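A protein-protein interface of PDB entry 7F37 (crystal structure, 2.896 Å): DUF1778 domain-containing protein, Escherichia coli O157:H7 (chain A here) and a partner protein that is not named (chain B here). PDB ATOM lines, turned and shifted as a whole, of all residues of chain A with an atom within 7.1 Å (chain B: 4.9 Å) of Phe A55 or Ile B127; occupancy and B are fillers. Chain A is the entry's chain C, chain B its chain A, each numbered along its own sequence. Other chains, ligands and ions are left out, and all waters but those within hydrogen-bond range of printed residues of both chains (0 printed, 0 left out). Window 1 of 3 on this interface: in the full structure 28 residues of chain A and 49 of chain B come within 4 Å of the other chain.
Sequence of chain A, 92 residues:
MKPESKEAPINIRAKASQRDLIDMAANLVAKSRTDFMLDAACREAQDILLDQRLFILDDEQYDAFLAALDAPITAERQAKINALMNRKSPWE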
ATOM      1  N   GLN A  52      -2.120 -12.494  30.302  1.00  0.00           N
ATOM      2  CA  GLN A  52      -0.799 -13.028  29.987  1.00  0.00           C
ATOM      3  C   GLN A  52      -0.510 -12.920  28.496  1.00  0.00           C
ATOM      4  O   GLN A  52      -1.228 -13.502  27.679  1.00  0.00           O
ATOM      5  CB  GLN A  52      -0.710 -14.482  30.425  1.00  0.00           C
ATOM      6  CG  GLN A  52       0.404 -15.270  29.744  1.00  0.00           C
ATOM      7  CD  GLN A  52       0.176 -16.758  29.885  1.00  0.00           C
ATOM      8  OE1 GLN A  52      -0.849 -17.175  30.415  1.00  0.00           O
ATOM      9  NE2 GLN A  52       1.122 -17.563  29.437  1.00  0.00           N
ATOM     10  N   ARG A  53       0.570 -12.230  28.144  1.00  0.00           N
ATOM     11  CA  ARG A  53       0.869 -11.914  26.752  1.00  0.00           C
ATOM     12  C   ARG A  53       2.185 -12.500  26.232  1.00  0.00           C
ATOM     13  O   ARG A  53       2.336 -12.659  25.012  1.00  0.00           O
ATOM     14  CB  ARG A  53       0.909 -10.385  26.549  1.00  0.00           C
ATOM     15  CG  ARG A  53      -0.339  -9.610  26.963  1.00  0.00           C
ATOM     16  CD  ARG A  53       0.031  -8.181  27.407  1.00  0.00           C
ATOM     17  NE  ARG A  53       0.602  -7.359  26.337  1.00  0.00           N
ATOM     18  CZ  ARG A  53       0.449  -6.039  26.242  1.00  0.00           C
ATOM     19  NH1 ARG A  53      -0.269  -5.377  27.151  1.00  0.00           N
ATOM     20  NH2 ARG A  53       1.000  -5.371  25.232  1.00  0.00           N
ATOM     21  N   LEU A  54       3.149 -12.808  27.101  1.00  0.00           N
ATOM     22  CA  LEU A  54       4.440 -13.331  26.662  1.00  0.00           C
ATOM     23  C   LEU A  54       4.529 -14.821  26.968  1.00  0.00           C
ATOM     24  O   LEU A  54       4.398 -15.234  28.126  1.00  0.00           O
ATOM     25  CB  LEU A  54       5.597 -12.592  27.326  1.00  0.00           C
ATOM     26  CG  LEU A  54       6.920 -12.870  26.636  1.00  0.00           C
ATOM     27  CD1 LEU A  54       6.774 -12.645  25.138  1.00  0.00           C
ATOM     28  CD2 LEU A  54       8.009 -12.002  27.198  1.00  0.00           C
ATOM     29  N   PHE A  55       4.743 -15.618  25.926  1.00  0.00           N
ATOM     30  CA  PHE A  55       4.911 -17.060  26.034  1.00  0.00           C
ATOM     31  C   PHE A  55       6.259 -17.387  25.431  1.00  0.00           C
ATOM     32  O   PHE A  55       6.432 -17.318  24.211  1.00  0.00           O
ATOM     33  CB  PHE A  55       3.824 -17.828  25.300  1.00  0.00           C
ATOM     34  CG  PHE A  55       2.458 -17.280  25.497  1.00  0.00           C
ATOM     35  CD1 PHE A  55       2.025 -16.188  24.761  1.00  0.00           C
ATOM     36  CD2 PHE A  55       1.588 -17.864  26.395  1.00  0.00           C
ATOM     37  CE1 PHE A  55       0.757 -15.677  24.922  1.00  0.00           C
ATOM     38  CE2 PHE A  55       0.307 -17.354  26.564  1.00  0.00           C
ATOM     39  CZ  PHE A  55      -0.105 -16.256  25.828  1.00  0.00           C
ATOM     40  N   ILE A  56       7.213 -17.739  26.277  1.00  0.00           N
ATOM     41  CA  ILE A  56       8.514 -18.189  25.823  1.00  0.00           C
ATOM     42  C   ILE A  56       8.489 -19.707  25.906  1.00  0.00           C
ATOM     43  O   ILE A  56       8.515 -20.287  26.993  1.00  0.00           O
ATOM     44  CB  ILE A  56       9.632 -17.572  26.650  1.00  0.00           C
ATOM     45  CG1 ILE A  56       9.534 -16.059  26.555  1.00  0.00           C
ATOM     46  CG2 ILE A  56      10.965 -18.014  26.133  1.00  0.00           C
ATOM     47  CD1 ILE A  56      10.545 -15.347  27.389  1.00  0.00           C
ATOM     48  N   LEU A  57       8.392 -20.352  24.755  1.00  0.00           N
ATOM     49  CA  LEU A  57       8.221 -21.790  24.659  1.00  0.00           C
ATOM     50  C   LEU A  57       9.494 -22.431  24.134  1.00  0.00           C
ATOM     51  O   LEU A  57      10.391 -21.752  23.628  1.00  0.00           O
ATOM     52  CB  LEU A  57       7.057 -22.138  23.738  1.00  0.00           C
ATOM     53  CG  LEU A  57       5.920 -21.156  23.888  1.00  0.00           C
ATOM     54  CD1 LEU A  57       5.013 -21.282  22.696  1.00  0.00           C
ATOM     55  CD2 LEU A  57       5.198 -21.462  25.195  1.00  0.00           C
ATOM     56  N   TYR A  62       7.152 -24.854  20.414  1.00  0.00           N
ATOM     57  CA  TYR A  62       6.991 -23.783  19.436  1.00  0.00           C
ATOM     58  C   TYR A  62       6.671 -24.351  18.051  1.00  0.00           C
ATOM     59  O   TYR A  62       5.827 -23.801  17.338  1.00  0.00           O
ATOM     60  CB  TYR A  62       8.250 -22.905  19.418  1.00  0.00           C
ATOM     61  CG  TYR A  62       8.122 -21.616  18.627  1.00  0.00           C
ATOM     62  CD1 TYR A  62       7.779 -20.425  19.249  1.00  0.00           C
ATOM     63  CD2 TYR A  62       8.361 -21.585  17.257  1.00  0.00           C
ATOM     64  CE1 TYR A  62       7.658 -19.241  18.524  1.00  0.00           C
ATOM     65  CE2 TYR A  62       8.241 -20.409  16.529  1.00  0.00           C
ATOM     66  CZ  TYR A  62       7.885 -19.246  17.170  1.00  0.00           C
ATOM     67  OH  TYR A  62       7.752 -18.080  16.461  1.00  0.00           O
ATOM     68  N   PHE A  65       3.265 -25.401  18.076  1.00  0.00           N
ATOM     69  CA  PHE A  65       2.468 -24.210  17.814  1.00  0.00           C
ATOM     70  C   PHE A  65       2.461 -23.867  16.327  1.00  0.00           C
ATOM     71  O   PHE A  65       1.392 -23.702  15.730  1.00  0.00           O
ATOM     72  CB  PHE A  65       3.008 -23.044  18.638  1.00  0.00           C
ATOM     73  CG  PHE A  65       2.416 -21.708  18.278  1.00  0.00           C
ATOM     74  CD1 PHE A  65       1.097 -21.406  18.591  1.00  0.00           C
ATOM     75  CD2 PHE A  65       3.190 -20.739  17.652  1.00  0.00           C
ATOM     76  CE1 PHE A  65       0.556 -20.173  18.265  1.00  0.00           C
ATOM     77  CE2 PHE A  65       2.656 -19.504  17.326  1.00  0.00           C
ATOM     78  CZ  PHE A  65       1.336 -19.221  17.635  1.00  0.00           C
ATOM     79  N   SER B  65       3.157 -11.783  22.279  1.00  0.00           N
ATOM     80  CA  SER B  65       4.174 -12.386  21.428  1.00  0.00           C
ATOM     81  C   SER B  65       4.579 -13.768  21.930  1.00  0.00           C
ATOM     82  O   SER B  65       4.684 -13.993  23.141  1.00  0.00           O
ATOM     83  CB  SER B  65       5.405 -11.486  21.342  1.00  0.00           C
ATOM     84  OG  SER B  65       6.354 -11.993  20.420  1.00  0.00           O
ATOM     85  N   ILE B  66       4.829 -14.677  20.983  1.00  0.00           N
ATOM     86  CA  ILE B  66       5.195 -16.055  21.268  1.00  0.00           C
ATOM     87  C   ILE B  66       6.583 -16.305  20.703  1.00  0.00           C
ATOM     88  O   ILE B  66       6.832 -16.018  19.529  1.00  0.00           O
ATOM     89  CB  ILE B  66       4.174 -17.028  20.669  1.00  0.00           C
ATOM     90  CG1 ILE B  66       2.893 -16.959  21.467  1.00  0.00           C
ATOM     91  CG2 ILE B  66       4.690 -18.443  20.703  1.00  0.00           C
ATOM     92  CD1 ILE B  66       1.690 -17.230  20.635  1.00  0.00           C
ATOM     93  N   GLN B  67       7.490 -16.843  21.537  1.00  0.00           N
ATOM     94  CA  GLN B  67       8.924 -16.757  21.271  1.00  0.00           C
ATOM     95  C   GLN B  67       9.629 -18.089  21.456  1.00  0.00           C
ATOM     96  O   GLN B  67       9.300 -18.855  22.362  1.00  0.00           O
ATOM     97  CB  GLN B  67       9.585 -15.713  22.170  1.00  0.00           C
ATOM     98  CG  GLN B  67       8.989 -14.339  21.955  1.00  0.00           C
ATOM     99  CD  GLN B  67      10.013 -13.251  21.923  1.00  0.00           C
ATOM    100  OE1 GLN B  67      11.149 -13.443  21.468  1.00  0.00           O
ATOM    101  NE2 GLN B  67       9.610 -12.074  22.360  1.00  0.00           N
ATOM    102  N   VAL B  85       1.022 -11.686  17.857  1.00  0.00           N
ATOM    103  CA  VAL B  85      -0.209 -12.383  18.184  1.00  0.00           C
ATOM    104  C   VAL B  85      -1.004 -11.484  19.116  1.00  0.00           C
ATOM    105  O   VAL B  85      -0.479 -10.497  19.619  1.00  0.00           O
ATOM    106  CB  VAL B  85       0.109 -13.767  18.816  1.00  0.00           C
ATOM    107  CG1 VAL B  85       0.611 -13.580  20.199  1.00  0.00           C
ATOM    108  CG2 VAL B  85      -1.096 -14.629  18.768  1.00  0.00           C
ATOM    109  N   VAL B  86      -2.295 -11.775  19.284  1.00  0.00           N
ATOM    110  CA  VAL B  86      -3.252 -10.873  19.940  1.00  0.00           C
ATOM    111  C   VAL B  86      -4.011 -11.654  21.007  1.00  0.00           C
ATOM    112  O   VAL B  86      -4.636 -12.683  20.705  1.00  0.00           O
ATOM    113  CB  VAL B  86      -4.250 -10.251  18.940  1.00  0.00           C
ATOM    114  CG1 VAL B  86      -5.371  -9.540  19.651  1.00  0.00           C
ATOM    115  CG2 VAL B  86      -3.550  -9.334  17.955  1.00  0.00           C
ATOM    116  N   VAL B  87      -3.985 -11.162  22.242  1.00  0.00           N
ATOM    117  CA  VAL B  87      -4.684 -11.811  23.350  1.00  0.00           C
ATOM    118  C   VAL B  87      -6.039 -11.146  23.520  1.00  0.00           C
ATOM    119  O   VAL B  87      -6.128  -9.915  23.576  1.00  0.00           O
ATOM    120  CB  VAL B  87      -3.867 -11.741  24.654  1.00  0.00           C
ATOM    121  CG1 VAL B  87      -4.527 -12.535  25.763  1.00  0.00           C
ATOM    122  CG2 VAL B  87      -2.495 -12.268  24.415  1.00  0.00           C
ATOM    123  N   LEU B  88      -7.094 -11.957  23.569  1.00  0.00           N
ATOM    124  CA  LEU B  88      -8.427 -11.496  23.952  1.00  0.00           C
ATOM    125  C   LEU B  88      -8.588 -11.784  25.440  1.00  0.00           C
ATOM    126  O   LEU B  88      -8.757 -12.932  25.860  1.00  0.00           O
ATOM    127  CB  LEU B  88      -9.502 -12.181  23.121  1.00  0.00           C
ATOM    128  CG  LEU B  88     -10.926 -11.977  23.644  1.00  0.00           C
ATOM    129  CD1 LEU B  88     -11.578 -10.698  23.074  1.00  0.00           C
ATOM    130  CD2 LEU B  88     -11.760 -13.209  23.342  1.00  0.00           C
ATOM    131  N   ALA B 125      -2.588 -15.196  15.420  1.00  0.00           N
ATOM    132  CA  ALA B 125      -3.674 -15.898  16.060  1.00  0.00           C
ATOM    133  C   ALA B 125      -4.333 -14.934  17.021  1.00  0.00           C
ATOM    134  O   ALA B 125      -3.764 -13.902  17.386  1.00  0.00           O
ATOM    135  CB  ALA B 125      -3.167 -17.137  16.788  1.00  0.00           C
ATOM    136  N   LEU B 126      -5.532 -15.266  17.430  1.00  0.00           N
ATOM    137  CA  LEU B 126      -6.188 -14.537  18.500  1.00  0.00           C
ATOM    138  C   LEU B 126      -6.180 -15.462  19.724  1.00  0.00           C
ATOM    139  O   LEU B 126      -7.023 -16.347  19.866  1.00  0.00           O
ATOM    140  CB  LEU B 126      -7.584 -14.086  18.072  1.00  0.00           C
ATOM    141  CG  LEU B 126      -8.577 -13.616  19.144  1.00  0.00           C
ATOM    142  CD1 LEU B 126      -8.213 -12.245  19.674  1.00  0.00           C
ATOM    143  CD2 LEU B 126     -10.010 -13.608  18.635  1.00  0.00           C
ATOM    144  N   ILE B 127      -5.207 -15.270  20.608  1.00  0.00           N
ATOM    145  CA  ILE B 127      -5.186 -16.081  21.808  1.00  0.00           C
ATOM    146  C   ILE B 127      -6.304 -15.649  22.754  1.00  0.00           C
ATOM    147  O   ILE B 127      -6.869 -14.558  22.652  1.00  0.00           O
ATOM    148  CB  ILE B 127      -3.815 -15.984  22.491  1.00  0.00           C
ATOM    149  CG1 ILE B 127      -2.714 -16.090  21.465  1.00  0.00           C
ATOM    150  CG2 ILE B 127      -3.613 -17.085  23.521  1.00  0.00           C
ATOM    151  CD1 ILE B 127      -1.394 -15.654  22.053  1.00  0.00           C
ATOM    152  N   VAL B 128      -6.612 -16.530  23.701  1.00  0.00           N
ATOM    153  CA  VAL B 128      -7.497 -16.207  24.803  1.00  0.00           C
ATOM    154  C   VAL B 128      -7.236 -17.240  25.880  1.00  0.00           C
ATOM    155  O   VAL B 128      -6.819 -18.362  25.589  1.00  0.00           O
ATOM    156  CB  VAL B 128      -8.973 -16.203  24.346  1.00  0.00           C
ATOM    157  CG1 VAL B 128      -9.333 -17.551  23.768  1.00  0.00           C
ATOM    158  CG2 VAL B 128      -9.887 -15.829  25.495  1.00  0.00           C
ATOM    159  N   HIS B 129      -7.468 -16.861  27.131  1.00  0.00           N
ATOM    160  CA  HIS B 129      -7.190 -17.729  28.268  1.00  0.00           C
ATOM    161  C   HIS B 129      -8.503 -18.048  28.967  1.00  0.00           C
ATOM    162  O   HIS B 129      -9.175 -17.148  29.477  1.00  0.00           O
ATOM    163  CB  HIS B 129      -6.201 -17.058  29.213  1.00  0.00           C
ATOM    164  CG  HIS B 129      -5.048 -16.402  28.512  1.00  0.00           C
ATOM    165  ND1 HIS B 129      -3.971 -17.113  28.022  1.00  0.00           N
ATOM    166  CD2 HIS B 129      -4.794 -15.100  28.234  1.00  0.00           C
ATOM    167  CE1 HIS B 129      -3.105 -16.277  27.474  1.00  0.00           C
ATOM    168  NE2 HIS B 129      -3.578 -15.049  27.592  1.00  0.00           N
ATOM    169  N   PHE B 144     -12.150 -21.880  18.484  1.00  0.00           N
ATOM    170  CA  PHE B 144     -10.829 -21.768  19.095  1.00  0.00           C
ATOM    171  C   PHE B 144     -10.247 -23.149  19.406  1.00  0.00           C
ATOM    172  O   PHE B 144     -10.837 -23.929  20.151  1.00  0.00           O
ATOM    173  CB  PHE B 144     -10.904 -20.928  20.360  1.00  0.00           C
ATOM    174  CG  PHE B 144     -10.927 -19.451  20.098  1.00  0.00           C
ATOM    175  CD1 PHE B 144     -12.050 -18.853  19.548  1.00  0.00           C
ATOM    176  CD2 PHE B 144      -9.822 -18.656  20.412  1.00  0.00           C
ATOM    177  CE1 PHE B 144     -12.072 -17.493  19.326  1.00  0.00           C
ATOM    178  CE2 PHE B 144      -9.846 -17.306  20.198  1.00  0.00           C
ATOM    179  CZ  PHE B 144     -10.962 -16.720  19.651  1.00  0.00           C
ATOM    180  N   PHE B 149       0.794 -25.599  23.873  1.00  0.00           N
ATOM    181  CA  PHE B 149       1.812 -25.200  24.840  1.00  0.00           C
ATOM    182  C   PHE B 149       1.277 -24.952  26.243  1.00  0.00           C
ATOM    183  O   PHE B 149       2.083 -24.875  27.173  1.00  0.00           O
ATOM    184  CB  PHE B 149       2.566 -23.943  24.363  1.00  0.00           C
ATOM    185  CG  PHE B 149       1.684 -22.746  24.098  1.00  0.00           C
ATOM    186  CD1 PHE B 149       1.356 -22.386  22.792  1.00  0.00           C
ATOM    187  CD2 PHE B 149       1.196 -21.968  25.147  1.00  0.00           C
ATOM    188  CE1 PHE B 149       0.552 -21.281  22.541  1.00  0.00           C
ATOM    189  CE2 PHE B 149       0.380 -20.861  24.905  1.00  0.00           C
ATOM    190  CZ  PHE B 149       0.063 -20.513  23.605  1.00  0.00           C
ATOM    191  N   GLN B 150      -0.034 -24.787  26.428  1.00  0.00           N
ATOM    192  CA  GLN B 150      -0.588 -24.793  27.780  1.00  0.00           C
ATOM    193  C   GLN B 150      -2.097 -24.961  27.703  1.00  0.00           C
ATOM    194  O   GLN B 150      -2.717 -24.697  26.673  1.00  0.00           O
ATOM    195  CB  GLN B 150      -0.195 -23.546  28.581  1.00  0.00           C
ATOM    196  CG  GLN B 150      -1.023 -22.338  28.405  1.00  0.00           C
ATOM    197  CD  GLN B 150      -0.289 -21.128  28.928  1.00  0.00           C
ATOM    198  OE1 GLN B 150      -0.697 -19.993  28.699  1.00  0.00           O
ATOM    199  NE2 GLN B 150       0.822 -21.365  29.625  1.00  0.00           N
ATOM    200  N   THR B 153      -5.126 -22.088  27.747  1.00  0.00           N
ATOM    201  CA  THR B 153      -5.026 -21.150  26.636  1.00  0.00           C
ATOM    202  C   THR B 153      -5.526 -21.778  25.337  1.00  0.00           C
ATOM    203  O   THR B 153      -4.944 -22.749  24.834  1.00  0.00           O
ATOM    204  CB  THR B 153      -3.584 -20.674  26.491  1.00  0.00           C
ATOM    205  OG1 THR B 153      -3.333 -19.642  27.450  1.00  0.00           O
ATOM    206  CG2 THR B 153      -3.294 -20.170  25.079  1.00  0.00           C
ATOM    207  N   LEU B 154      -6.606 -21.211  24.800  1.00  0.00           N
ATOM    208  CA  LEU B 154      -7.106 -21.520  23.469  1.00  0.00           C
ATOM    209  C   LEU B 154      -6.650 -20.438  22.498  1.00  0.00           C
ATOM    210  O   LEU B 154      -6.277 -19.329  22.903  1.00  0.00           O
ATOM    211  CB  LEU B 154      -8.629 -21.605  23.465  1.00  0.00           C
ATOM    212  CG  LEU B 154      -9.167 -22.171  24.773  1.00  0.00           C
ATOM    213  CD1 LEU B 154     -10.692 -22.175  24.753  1.00  0.00           C
ATOM    214  CD2 LEU B 154      -8.589 -23.582  25.056  1.00  0.00           C
ATOM    215  N   LEU B 155      -6.693 -20.763  21.205  1.00  0.00           N
ATOM    216  CA  LEU B 155      -6.322 -19.784  20.204  1.00  0.00           C
ATOM    217  C   LEU B 155      -7.013 -20.100  18.900  1.00  0.00           C
ATOM    218  O   LEU B 155      -7.365 -21.246  18.622  1.00  0.00           O
ATOM    219  CB  LEU B 155      -4.816 -19.740  20.006  1.00  0.00           C
ATOM    220  CG  LEU B 155      -4.155 -20.806  19.159  1.00  0.00           C
ATOM    221  CD1 LEU B 155      -2.834 -20.239  18.762  1.00  0.00           C
ATOM    222  CD2 LEU B 155      -3.952 -22.060  19.964  1.00  0.00           C
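The backbone NH of Leu A57 is in hydrogen-bond range of the backbone carbonyl oxygen of Gln B67.
O of Ser B65 lies within hydrogen-bond range of N of Phe A55, at 3.2 Å.
The side-chain amide oxygen (OE1) of Gln B150 sits at hydrogen-bond distance from the side-chain amide nitrogen (NE2) of Gln A52 (3.1 Å).
A ring nitrogen (NE2) of His B129 lies within hydrogen-bond range of the backbone carbonyl oxygen of Gln A52.
The backbone carbonyl oxygen (O) of Phe A55 sits at hydrogen-bond distance from the backbone NH (N) of Gln B67 (2.9 Å).
N of Ser B65 lies within hydrogen-bond range of O of Arg A53.
A ring nitrogen (ND1) of His B129 sits at hydrogen-bond distance from the side-chain hydroxyl (OG1) of Thr B153 (2.7 Å).
N of Leu B88 is in hydrogen-bond range of O of Ile B127 (2.8 Å).
O of Val B86 is in hydrogen-bond range of N of Ile B127 (2.7 Å).
OE1 of Gln B150 sits at hydrogen-bond distance from OG1 of Thr B153 (2.9 Å).
Among the printed residues, merely in contact across the chains: Gln A52 with Val B87 (3.7 Å), Leu A54 with Ser B65 (3.2 Å), Phe A55 with Ile B66 (3.4 Å), Phe A55 with Ile B127 (3.6 Å), Phe A55 with His B129 (3.4 Å), Phe A55 with Phe B149 (3.6 Å), Phe A55 with Gln B150 (3.5 Å), Ile A56 with Gln B67 (3.6 Å), Leu A57 with Ile B66 (3.5 Å), Leu A57 with Phe B149 (3.7 Å), Tyr A62 with Ile B66 (3.5 Å), Tyr A62 with Gln B67 (3.7 Å), Phe A65 with Ile B66 (3.6 Å), Phe A65 with Phe B149 (3.99 Å) and Phe A65 with Leu B155 (3.4 Å).
Phe A55 touches just these residues of chain B: Ser B65, Ile B66, Gln B67, Ile B127, His B129, Phe B149 and Gln B150.
Printed residues of chain B within 4 Å of Phe A65: Ile B66, Phe B149 and Leu B155.
Of the printed residues of chain A, Val B87 touches Gln A52.
Ile B127 touches one residue of chain A.
Val B128 touches none of the printed residues of chain A.
Thr B153 touches none of the printed residues of chain A.
The nearest residue of chain B that does not touch Phe A55 is Thr B153 (4.4 Å).
Of the 18 printed residues of chain B, 9 touch a printed residue of chain A.
Of the 8 printed residues of chain A, 8 touch a printed residue of chain B.
Hydrophobic or aromatic side chains of chain A within 4 Å of the printed part of chain B: Leu A54, Phe A55, Leu A57, Tyr A62 and Phe A65.
Among the printed residues, 21 pairs touch across the chains.
Among the printed residues, no Asp or Glu carboxylate lies within 4 Å of a Lys or Arg side-chain nitrogen of the other chain.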
